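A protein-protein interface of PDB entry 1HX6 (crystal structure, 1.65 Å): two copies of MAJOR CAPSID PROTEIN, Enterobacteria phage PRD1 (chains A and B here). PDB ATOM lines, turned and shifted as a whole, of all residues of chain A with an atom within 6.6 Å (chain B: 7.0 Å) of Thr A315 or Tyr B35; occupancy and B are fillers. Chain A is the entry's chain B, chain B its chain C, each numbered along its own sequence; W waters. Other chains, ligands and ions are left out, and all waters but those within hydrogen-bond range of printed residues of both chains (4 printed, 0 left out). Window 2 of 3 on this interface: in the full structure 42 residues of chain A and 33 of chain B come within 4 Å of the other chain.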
ATOM      1  N   SER A 306     -20.641  10.202  16.227  1.00  0.00           N
ATOM      2  CA  SER A 306     -19.892  10.915  15.204  1.00  0.00           C
ATOM      3  C   SER A 306     -18.511  10.311  14.980  1.00  0.00           C
ATOM      4  O   SER A 306     -18.085   9.398  15.693  1.00  0.00           O
ATOM      5  CB  SER A 306     -19.738  12.395  15.621  1.00  0.00           C
ATOM      6  OG  SER A 306     -19.257  13.187  14.546  1.00  0.00           O
ATOM      7  N   GLN A 307     -17.843  10.815  13.948  1.00  0.00           N
ATOM      8  CA  GLN A 307     -16.458  10.474  13.641  1.00  0.00           C
ATOM      9  C   GLN A 307     -15.870  11.883  13.590  1.00  0.00           C
ATOM     10  O   GLN A 307     -16.433  12.772  12.951  1.00  0.00           O
ATOM     11  CB  GLN A 307     -16.314   9.752  12.302  1.00  0.00           C
ATOM     12  CG  GLN A 307     -16.600   8.254  12.407  1.00  0.00           C
ATOM     13  CD  GLN A 307     -16.162   7.478  11.173  1.00  0.00           C
ATOM     14  OE1 GLN A 307     -16.462   7.865  10.046  1.00  0.00           O
ATOM     15  NE2 GLN A 307     -15.458   6.372  11.383  1.00  0.00           N
ATOM     16  N   ARG A 308     -14.756  12.094  14.273  1.00  0.00           N
ATOM     17  CA  ARG A 308     -14.182  13.431  14.359  1.00  0.00           C
ATOM     18  C   ARG A 308     -12.671  13.468  14.205  1.00  0.00           C
ATOM     19  O   ARG A 308     -11.969  12.583  14.688  1.00  0.00           O
ATOM     20  CB  ARG A 308     -14.589  14.015  15.714  1.00  0.00           C
ATOM     21  CG  ARG A 308     -13.951  15.319  16.112  1.00  0.00           C
ATOM     22  CD  ARG A 308     -14.413  15.668  17.521  1.00  0.00           C
ATOM     23  NE  ARG A 308     -15.872  15.711  17.607  1.00  0.00           N
ATOM     24  CZ  ARG A 308     -16.555  15.654  18.747  1.00  0.00           C
ATOM     25  NH1 ARG A 308     -15.911  15.547  19.904  1.00  0.00           N
ATOM     26  NH2 ARG A 308     -17.882  15.715  18.729  1.00  0.00           N
ATOM     27  N   THR A 309     -12.181  14.504  13.532  1.00  0.00           N
ATOM     28  CA  THR A 309     -10.749  14.675  13.321  1.00  0.00           C
ATOM     29  C   THR A 309     -10.209  15.769  14.232  1.00  0.00           C
ATOM     30  O   THR A 309     -10.967  16.591  14.747  1.00  0.00           O
ATOM     31  CB  THR A 309     -10.436  15.089  11.873  1.00  0.00           C
ATOM     32  OG1 THR A 309     -11.167  16.279  11.554  1.00  0.00           O
ATOM     33  CG2 THR A 309     -10.820  13.990  10.904  1.00  0.00           C
ATOM     34  N   SER A 313     -13.757  19.030  13.856  1.00  0.00           N
ATOM     35  CA  SER A 313     -14.581  18.782  12.683  1.00  0.00           C
ATOM     36  C   SER A 313     -15.173  17.383  12.626  1.00  0.00           C
ATOM     37  O   SER A 313     -14.449  16.393  12.481  1.00  0.00           O
ATOM     38  CB  SER A 313     -13.780  19.033  11.399  1.00  0.00           C
ATOM     39  OG  SER A 313     -13.809  20.403  11.041  1.00  0.00           O
ATOM     40  N   ASP A 314     -16.497  17.321  12.746  1.00  0.00           N
ATOM     41  CA  ASP A 314     -17.229  16.065  12.663  1.00  0.00           C
ATOM     42  C   ASP A 314     -17.552  15.882  11.186  1.00  0.00           C
ATOM     43  O   ASP A 314     -17.924  16.841  10.503  1.00  0.00           O
ATOM     44  CB  ASP A 314     -18.545  16.144  13.444  1.00  0.00           C
ATOM     45  CG  ASP A 314     -18.338  16.206  14.942  1.00  0.00           C
ATOM     46  OD1 ASP A 314     -17.825  15.230  15.515  1.00  0.00           O
ATOM     47  OD2 ASP A 314     -18.698  17.239  15.550  1.00  0.00           O
ATOM     48  N   THR A 315     -17.401  14.662  10.685  1.00  0.00           N
ATOM     49  CA  THR A 315     -17.704  14.393   9.287  1.00  0.00           C
ATOM     50  C   THR A 315     -19.104  13.797   9.168  1.00  0.00           C
ATOM     51  O   THR A 315     -19.679  13.737   8.076  1.00  0.00           O
ATOM     52  CB  THR A 315     -16.693  13.426   8.688  1.00  0.00           C
ATOM     53  OG1 THR A 315     -16.579  12.281   9.542  1.00  0.00           O
ATOM     54  CG2 THR A 315     -15.341  14.103   8.543  1.00  0.00           C
ATOM     55  N   ARG A 316     -19.646  13.343  10.293  1.00  0.00           N
ATOM     56  CA  ARG A 316     -20.989  12.776  10.301  1.00  0.00           C
ATOM     57  C   ARG A 316     -21.561  12.683  11.709  1.00  0.00           C
ATOM     58  O   ARG A 316     -21.834  11.596  12.218  1.00  0.00           O
ATOM     59  CB  ARG A 316     -21.014  11.397   9.618  1.00  0.00           C
ATOM     60  CG  ARG A 316     -20.005  10.365  10.128  1.00  0.00           C
ATOM     61  CD  ARG A 316     -20.234   9.021   9.412  1.00  0.00           C
ATOM     62  NE  ARG A 316     -21.439   8.363   9.920  1.00  0.00           N
ATOM     63  CZ  ARG A 316     -22.014   7.291   9.380  1.00  0.00           C
ATOM     64  NH1 ARG A 316     -21.507   6.737   8.287  1.00  0.00           N
ATOM     65  NH2 ARG A 316     -23.091   6.760   9.953  1.00  0.00           N
ATOM     66  N   LYS A 317     -21.729  13.833  12.335  1.00  0.00           N
ATOM     67  CA  LYS A 317     -22.300  13.900  13.676  1.00  0.00           C
ATOM     68  C   LYS A 317     -23.814  13.765  13.477  1.00  0.00           C
ATOM     69  O   LYS A 317     -24.463  14.690  12.979  1.00  0.00           O
ATOM     70  CB  LYS A 317     -21.961  15.243  14.299  1.00  0.00           C
ATOM     71  CG  LYS A 317     -22.600  15.475  15.652  1.00  0.00           C
ATOM     72  CD  LYS A 317     -22.260  16.882  16.133  1.00  0.00           C
ATOM     73  CE  LYS A 317     -22.918  17.201  17.457  1.00  0.00           C
ATOM     74  NZ  LYS A 317     -22.642  18.620  17.854  1.00  0.00           N
ATOM     75  N   ASN A 344     -16.450   2.880   6.305  1.00  0.00           N
ATOM     76  CA  ASN A 344     -15.401   3.791   5.816  1.00  0.00           C
ATOM     77  C   ASN A 344     -14.571   3.037   4.771  1.00  0.00           C
ATOM     78  O   ASN A 344     -13.374   3.280   4.625  1.00  0.00           O
ATOM     79  CB  ASN A 344     -14.479   4.235   6.957  1.00  0.00           C
ATOM     80  CG  ASN A 344     -15.186   5.089   7.994  1.00  0.00           C
ATOM     81  OD1 ASN A 344     -15.582   6.237   7.727  1.00  0.00           O
ATOM     82  ND2 ASN A 344     -15.347   4.541   9.182  1.00  0.00           N
ATOM     83  N   LYS A 347     -12.970   5.236   1.798  1.00  0.00           N
ATOM     84  CA  LYS A 347     -11.969   6.171   2.321  1.00  0.00           C
ATOM     85  C   LYS A 347     -11.681   5.760   3.757  1.00  0.00           C
ATOM     86  O   LYS A 347     -12.180   6.360   4.701  1.00  0.00           O
ATOM     87  CB  LYS A 347     -12.503   7.609   2.281  1.00  0.00           C
ATOM     88  CG  LYS A 347     -12.707   8.156   0.864  1.00  0.00           C
ATOM     89  CD  LYS A 347     -13.307   9.563   0.880  1.00  0.00           C
ATOM     90  CE  LYS A 347     -13.509  10.102  -0.544  1.00  0.00           C
ATOM     91  NZ  LYS A 347     -12.218  10.323  -1.253  1.00  0.00           N
ATOM     92  N   PRO A 348     -10.858   4.720   3.934  1.00  0.00           N
ATOM     93  CA  PRO A 348     -10.496   4.196   5.255  1.00  0.00           C
ATOM     94  C   PRO A 348      -9.921   5.244   6.185  1.00  0.00           C
ATOM     95  O   PRO A 348      -9.192   6.134   5.744  1.00  0.00           O
ATOM     96  CB  PRO A 348      -9.471   3.115   4.931  1.00  0.00           C
ATOM     97  CG  PRO A 348      -9.827   2.698   3.529  1.00  0.00           C
ATOM     98  CD  PRO A 348     -10.132   4.006   2.870  1.00  0.00           C
ATOM     99  N   ILE A 349     -10.263   5.149   7.466  1.00  0.00           N
ATOM    100  CA  ILE A 349      -9.730   6.084   8.445  1.00  0.00           C
ATOM    101  C   ILE A 349      -8.246   5.739   8.558  1.00  0.00           C
ATOM    102  O   ILE A 349      -7.883   4.595   8.829  1.00  0.00           O
ATOM    103  CB  ILE A 349     -10.400   5.919   9.823  1.00  0.00           C
ATOM    104  CG1 ILE A 349     -11.917   6.131   9.707  1.00  0.00           C
ATOM    105  CG2 ILE A 349      -9.768   6.882  10.815  1.00  0.00           C
ATOM    106  CD1 ILE A 349     -12.325   7.454   9.089  1.00  0.00           C
ATOM    107  N   GLN A 353      -3.404  10.390   7.000  1.00  0.00           N
ATOM    108  CA  GLN A 353      -4.112  11.197   6.008  1.00  0.00           C
ATOM    109  C   GLN A 353      -4.532  12.536   6.611  1.00  0.00           C
ATOM    110  O   GLN A 353      -4.483  13.572   5.946  1.00  0.00           O
ATOM    111  CB  GLN A 353      -5.344  10.440   5.510  1.00  0.00           C
ATOM    112  CG  GLN A 353      -5.792  10.827   4.116  1.00  0.00           C
ATOM    113  CD  GLN A 353      -6.998  10.028   3.654  1.00  0.00           C
ATOM    114  OE1 GLN A 353      -7.367  10.065   2.478  1.00  0.00           O
ATOM    115  NE2 GLN A 353      -7.626   9.308   4.582  1.00  0.00           N
ATOM    116  N   TYR A 354      -4.964  12.497   7.869  1.00  0.00           N
ATOM    117  CA  TYR A 354      -5.360  13.696   8.601  1.00  0.00           C
ATOM    118  C   TYR A 354      -4.838  13.532  10.022  1.00  0.00           C
ATOM    119  O   TYR A 354      -4.083  12.603  10.298  1.00  0.00           O
ATOM    120  CB  TYR A 354      -6.882  13.868   8.616  1.00  0.00           C
ATOM    121  CG  TYR A 354      -7.480  14.176   7.257  1.00  0.00           C
ATOM    122  CD1 TYR A 354      -7.875  13.148   6.394  1.00  0.00           C
ATOM    123  CD2 TYR A 354      -7.619  15.497   6.817  1.00  0.00           C
ATOM    124  CE1 TYR A 354      -8.393  13.427   5.124  1.00  0.00           C
ATOM    125  CE2 TYR A 354      -8.135  15.789   5.546  1.00  0.00           C
ATOM    126  CZ  TYR A 354      -8.519  14.750   4.706  1.00  0.00           C
ATOM    127  OH  TYR A 354      -9.021  15.023   3.452  1.00  0.00           O
ATOM    128  N   VAL B  30     -12.226  15.377  -7.961  1.00  0.00           N
ATOM    129  CA  VAL B  30     -12.961  15.941  -6.835  1.00  0.00           C
ATOM    130  C   VAL B  30     -13.363  14.820  -5.874  1.00  0.00           C
ATOM    131  O   VAL B  30     -13.174  14.939  -4.668  1.00  0.00           O
ATOM    132  CB  VAL B  30     -14.222  16.691  -7.312  1.00  0.00           C
ATOM    133  CG1 VAL B  30     -15.233  16.822  -6.167  1.00  0.00           C
ATOM    134  CG2 VAL B  30     -13.829  18.078  -7.811  1.00  0.00           C
ATOM    135  N   LEU B  31     -13.895  13.728  -6.411  1.00  0.00           N
ATOM    136  CA  LEU B  31     -14.316  12.610  -5.566  1.00  0.00           C
ATOM    137  C   LEU B  31     -13.149  11.968  -4.811  1.00  0.00           C
ATOM    138  O   LEU B  31     -13.287  11.588  -3.649  1.00  0.00           O
ATOM    139  CB  LEU B  31     -15.033  11.550  -6.409  1.00  0.00           C
ATOM    140  CG  LEU B  31     -16.376  11.966  -7.020  1.00  0.00           C
ATOM    141  CD1 LEU B  31     -16.886  10.864  -7.930  1.00  0.00           C
ATOM    142  CD2 LEU B  31     -17.385  12.259  -5.915  1.00  0.00           C
ATOM    143  N   GLN B  32     -11.997  11.856  -5.469  1.00  0.00           N
ATOM    144  CA  GLN B  32     -10.826  11.247  -4.831  1.00  0.00           C
ATOM    145  C   GLN B  32     -10.182  12.142  -3.782  1.00  0.00           C
ATOM    146  O   GLN B  32      -9.793  11.669  -2.725  1.00  0.00           O
ATOM    147  CB  GLN B  32      -9.752  10.895  -5.870  1.00  0.00           C
ATOM    148  CG  GLN B  32     -10.198   9.964  -6.979  1.00  0.00           C
ATOM    149  CD  GLN B  32     -10.872   8.710  -6.460  1.00  0.00           C
ATOM    150  OE1 GLN B  32     -10.308   7.973  -5.637  1.00  0.00           O
ATOM    151  NE2 GLN B  32     -12.090   8.454  -6.940  1.00  0.00           N
ATOM    152  N   GLN B  33     -10.075  13.435  -4.083  1.00  0.00           N
ATOM    153  CA  GLN B  33      -9.428  14.405  -3.196  1.00  0.00           C
ATOM    154  C   GLN B  33     -10.232  15.034  -2.055  1.00  0.00           C
ATOM    155  O   GLN B  33      -9.684  15.305  -0.982  1.00  0.00           O
ATOM    156  CB  GLN B  33      -8.841  15.541  -4.036  1.00  0.00           C
ATOM    157  CG  GLN B  33      -7.784  15.099  -5.026  1.00  0.00           C
ATOM    158  CD  GLN B  33      -6.583  14.497  -4.335  1.00  0.00           C
ATOM    159  OE1 GLN B  33      -6.019  15.098  -3.419  1.00  0.00           O
ATOM    160  NE2 GLN B  33      -6.183  13.306  -4.767  1.00  0.00           N
ATOM    161  N   SER B  34     -11.513  15.296  -2.288  1.00  0.00           N
ATOM    162  CA  SER B  34     -12.356  15.915  -1.266  1.00  0.00           C
ATOM    163  C   SER B  34     -12.827  14.873  -0.260  1.00  0.00           C
ATOM    164  O   SER B  34     -12.684  13.672  -0.488  1.00  0.00           O
ATOM    165  CB  SER B  34     -13.578  16.565  -1.921  1.00  0.00           C
ATOM    166  OG  SER B  34     -14.421  15.581  -2.498  1.00  0.00           O
ATOM    167  N   TYR B  35     -13.380  15.325   0.860  1.00  0.00           N
ATOM    168  CA  TYR B  35     -13.899  14.378   1.846  1.00  0.00           C
ATOM    169  C   TYR B  35     -15.370  14.686   2.080  1.00  0.00           C
ATOM    170  O   TYR B  35     -15.735  15.833   2.349  1.00  0.00           O
ATOM    171  CB  TYR B  35     -13.153  14.474   3.177  1.00  0.00           C
ATOM    172  CG  TYR B  35     -13.413  13.274   4.076  1.00  0.00           C
ATOM    173  CD1 TYR B  35     -12.760  12.052   3.852  1.00  0.00           C
ATOM    174  CD2 TYR B  35     -14.340  13.342   5.121  1.00  0.00           C
ATOM    175  CE1 TYR B  35     -13.025  10.930   4.646  1.00  0.00           C
ATOM    176  CE2 TYR B  35     -14.611  12.222   5.921  1.00  0.00           C
ATOM    177  CZ  TYR B  35     -13.950  11.021   5.677  1.00  0.00           C
ATOM    178  OH  TYR B  35     -14.212   9.917   6.467  1.00  0.00           O
ATOM    179  N   PRO B  36     -16.235  13.667   1.973  1.00  0.00           N
ATOM    180  CA  PRO B  36     -17.668  13.880   2.182  1.00  0.00           C
ATOM    181  C   PRO B  36     -18.015  14.199   3.638  1.00  0.00           C
ATOM    182  O   PRO B  36     -17.426  13.649   4.573  1.00  0.00           O
ATOM    183  CB  PRO B  36     -18.277  12.565   1.710  1.00  0.00           C
ATOM    184  CG  PRO B  36     -17.231  11.563   2.106  1.00  0.00           C
ATOM    185  CD  PRO B  36     -15.956  12.252   1.660  1.00  0.00           C
ATOM    186  N   VAL B  37     -18.973  15.099   3.816  1.00  0.00           N
ATOM    187  CA  VAL B  37     -19.426  15.504   5.140  1.00  0.00           C
ATOM    188  C   VAL B  37     -20.945  15.566   5.125  1.00  0.00           C
ATOM    189  O   VAL B  37     -21.547  15.900   4.109  1.00  0.00           O
ATOM    190  CB  VAL B  37     -18.932  16.929   5.504  1.00  0.00           C
ATOM    191  CG1 VAL B  37     -19.528  17.365   6.857  1.00  0.00           C
ATOM    192  CG2 VAL B  37     -17.411  16.969   5.545  1.00  0.00           C
ATOM    193  N   ILE B  38     -21.564  15.196   6.237  1.00  0.00           N
ATOM    194  CA  ILE B  38     -23.006  15.326   6.355  1.00  0.00           C
ATOM    195  C   ILE B  38     -23.173  15.971   7.720  1.00  0.00           C
ATOM    196  O   ILE B  38     -22.680  15.452   8.719  1.00  0.00           O
ATOM    197  CB  ILE B  38     -23.773  13.971   6.280  1.00  0.00           C
ATOM    198  CG1 ILE B  38     -25.280  14.254   6.382  1.00  0.00           C
ATOM    199  CG2 ILE B  38     -23.332  13.027   7.393  1.00  0.00           C
ATOM    200  CD1 ILE B  38     -26.194  13.076   6.021  1.00  0.00           C
ATOM    201  N   GLN B  39     -23.818  17.134   7.768  1.00  0.00           N
ATOM    202  CA  GLN B  39     -23.988  17.800   9.051  1.00  0.00           C
ATOM    203  C   GLN B  39     -25.315  18.523   9.175  1.00  0.00           C
ATOM    204  O   GLN B  39     -25.861  19.011   8.184  1.00  0.00           O
ATOM    205  CB  GLN B  39     -22.851  18.788   9.298  1.00  0.00           C
ATOM    206  CG  GLN B  39     -22.909  20.042   8.489  1.00  0.00           C
ATOM    207  CD  GLN B  39     -21.808  21.012   8.883  1.00  0.00           C
ATOM    208  OE1 GLN B  39     -21.655  21.355  10.057  1.00  0.00           O
ATOM    209  NE2 GLN B  39     -21.034  21.452   7.905  1.00  0.00           N
ATOM    210  N   TYR B 235     -22.301  17.335   1.680  1.00  0.00           N
ATOM    211  CA  TYR B 235     -21.449  18.064   0.747  1.00  0.00           C
ATOM    212  C   TYR B 235     -20.022  17.534   0.730  1.00  0.00           C
ATOM    213  O   TYR B 235     -19.658  16.652   1.516  1.00  0.00           O
ATOM    214  CB  TYR B 235     -21.445  19.557   1.111  1.00  0.00           C
ATOM    215  CG  TYR B 235     -20.895  19.870   2.487  1.00  0.00           C
ATOM    216  CD1 TYR B 235     -21.721  19.839   3.609  1.00  0.00           C
ATOM    217  CD2 TYR B 235     -19.549  20.209   2.670  1.00  0.00           C
ATOM    218  CE1 TYR B 235     -21.229  20.142   4.881  1.00  0.00           C
ATOM    219  CE2 TYR B 235     -19.047  20.512   3.939  1.00  0.00           C
ATOM    220  CZ  TYR B 235     -19.893  20.476   5.038  1.00  0.00           C
ATOM    221  OH  TYR B 235     -19.421  20.770   6.299  1.00  0.00           O
ATOM    222  N   LEU B 236     -19.222  18.073  -0.187  1.00  0.00           N
ATOM    223  CA  LEU B 236     -17.820  17.682  -0.315  1.00  0.00           C
ATOM    224  C   LEU B 236     -16.959  18.870   0.088  1.00  0.00           C
ATOM    225  O   LEU B 236     -17.127  19.976  -0.434  1.00  0.00           O
ATOM    226  CB  LEU B 236     -17.506  17.262  -1.755  1.00  0.00           C
ATOM    227  CG  LEU B 236     -18.355  16.105  -2.297  1.00  0.00           C
ATOM    228  CD1 LEU B 236     -18.007  15.851  -3.765  1.00  0.00           C
ATOM    229  CD2 LEU B 236     -18.117  14.849  -1.448  1.00  0.00           C
ATOM    230  N   ASP B 237     -16.052  18.632   1.029  1.00  0.00           N
ATOM    231  CA  ASP B 237     -15.168  19.671   1.536  1.00  0.00           C
ATOM    232  C   ASP B 237     -13.719  19.452   1.084  1.00  0.00           C
ATOM    233  O   ASP B 237     -13.388  18.402   0.532  1.00  0.00           O
ATOM    234  CB  ASP B 237     -15.231  19.688   3.063  1.00  0.00           C
ATOM    235  CG  ASP B 237     -15.203  21.085   3.622  1.00  0.00           C
ATOM    236  OD1 ASP B 237     -15.131  22.041   2.819  1.00  0.00           O
ATOM    237  OD2 ASP B 237     -15.257  21.231   4.860  1.00  0.00           O
ATOM    238  N   GLN B 238     -12.873  20.450   1.330  1.00  0.00           N
ATOM    239  CA  GLN B 238     -11.464  20.393   0.949  1.00  0.00           C
ATOM    240  C   GLN B 238     -11.355  20.089  -0.541  1.00  0.00           C
ATOM    241  O   GLN B 238     -10.733  19.107  -0.948  1.00  0.00           O
ATOM    242  CB  GLN B 238     -10.736  19.316   1.755  1.00  0.00           C
ATOM    243  CG  GLN B 238     -10.905  19.451   3.259  1.00  0.00           C
ATOM    244  CD  GLN B 238     -10.080  18.440   4.027  1.00  0.00           C
ATOM    245  OE1 GLN B 238     -10.087  17.251   3.708  1.00  0.00           O
ATOM    246  NE2 GLN B 238      -9.373  18.904   5.051  1.00  0.00           N
ATOM    247  N   LEU B 239     -11.977  20.943  -1.348  1.00  0.00           N
ATOM    248  CA  LEU B 239     -11.973  20.781  -2.793  1.00  0.00           C
ATOM    249  C   LEU B 239     -10.559  20.890  -3.349  1.00  0.00           C
ATOM    250  O   LEU B 239      -9.806  21.794  -2.982  1.00  0.00           O
ATOM    251  CB  LEU B 239     -12.890  21.828  -3.434  1.00  0.00           C
ATOM    252  CG  LEU B 239     -14.367  21.755  -3.017  1.00  0.00           C
ATOM    253  CD1 LEU B 239     -15.163  22.838  -3.733  1.00  0.00           C
ATOM    254  CD2 LEU B 239     -14.926  20.388  -3.352  1.00  0.00           C
HETATM  255  O   HOH W   1     -14.707   7.276   5.100  1.00  0.00           O
HETATM  256  O   HOH W   2     -15.970  10.043   8.517  1.00  0.00           O
HETATM  257  O   HOH W   3     -20.979  16.511  10.980  1.00  0.00           O
HETATM  258  O   HOH W   4     -19.209  11.698   6.292  1.00  0.00           O
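The side-chain amino group (NZ) of Lys A347 sits at hydrogen-bond distance from the backbone carbonyl oxygen (O) of Gln B32, at 3.1 Å. The backbone NH of Ile B38 sits at hydrogen-bond distance from the backbone carbonyl oxygen of Thr A315, at 3.0 Å. O of Leu B31 sits at hydrogen-bond distance from NZ of Lys A347 (2.9 Å). OH of Tyr A354 is in hydrogen-bond range of OE1 of Gln B238. The side-chain amino group (NZ) of Lys A347 lies within hydrogen-bond range of the backbone carbonyl oxygen (O) of Ser B34.
N of Val B37 is in hydrogen-bond range of O of Tyr B235, at 2.9 Å. The backbone carbonyl oxygen (O) of Gln A307 lies within hydrogen-bond range of the backbone NH (N) of Thr A315 (3.1 Å). The side-chain hydroxyl (OG) of Ser B34 sits at hydrogen-bond distance from the backbone carbonyl oxygen (O) of Val B30 (2.6 Å). N of Tyr B35 is in hydrogen-bond range of O of Asp B237 (3.1 Å).
CE2 of Tyr B35 touches CG2 of Thr A315, 3.3 Å away. Val B37 touches Thr A315 (CA to O, 3.4 Å). Ile B38 touches Arg A316 (O to CA, 3.5 Å). Lys A347 touches Tyr B35. CD of Lys A347 touches CD of Pro B36, 3.9 Å away.
Of chain B, only Tyr B35 (3.3 Å), Val B37 (3.4 Å) and Ile B38 (3.0 Å) come within 4 Å of Thr A315. Tyr B35 touches two residues of chain A. Printed residues of chain B within 4 Å of Arg A316: Ile B38 (3.5 Å). Printed residues of chain B within 4 Å of Lys A347: Leu B31 (2.9 Å), Gln B32 (3.1 Å), Ser B34 (3.5 Å), Tyr B35 (3.9 Å) and Pro B36 (3.9 Å). Printed residues of chain A within 4 Å of Ile B38: Thr A315 (3.0 Å) and Arg A316 (3.5 Å). Of the printed residues of chain A, Gln B238 touches Tyr A354. The nearest residue of chain B that does not touch Thr A315 is Pro B36 (4.2 Å). The nearest residue of chain A that does not touch Tyr B35 is Ile A349 (4.1 Å). The nearest printed residue of chain A that does not touch Pro B36 is Thr A315 (4.2 Å).
Of the 15 printed residues of chain A, 4 touch a printed residue of chain B. Hydrophobic or aromatic side chains of chain A that line the printed part of chain B: Tyr A354. Printed residues of chain B that touch a printed residue of chain A: Leu B31, Gln B32, Ser B34, Tyr B35, Pro B36, Val B37, Ile B38 and Gln B238. Hydrophobic or aromatic side chains of chain B within 4 Å of the printed part of chain A: Tyr B35, Pro B36, Val B37 and Ile B38. Among the printed residues, 10 pairs touch across the chains.
No position is printed for both chains. Of the 10 pairs that touch across the chains among the printed residues, none has its exchanged pair printed and touching as well.
Water W2 lies within hydrogen-bond range of the side-chain hydroxyl of Thr A315 (2.5 Å), the side-chain hydroxyl of Tyr B35 (2.7 Å) and the side-chain amide oxygen of Gln A307 (2.7 Å). Water W1 lies within hydrogen-bond range of the backbone carbonyl oxygen of Lys A347, the side-chain amide oxygen of Asn A344 and the side-chain hydroxyl of Tyr B35. Water W4 bridges O of Thr A315 (2.7 Å) and O of Pro B36 (3.2 Å). Water W3 lies within hydrogen-bond range of the backbone carbonyl oxygen of Ile B38 (3.0 Å), the backbone NH of Lys A317 (3.1 Å) and the backbone carbonyl oxygen of Asp A314 (3.1 Å).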
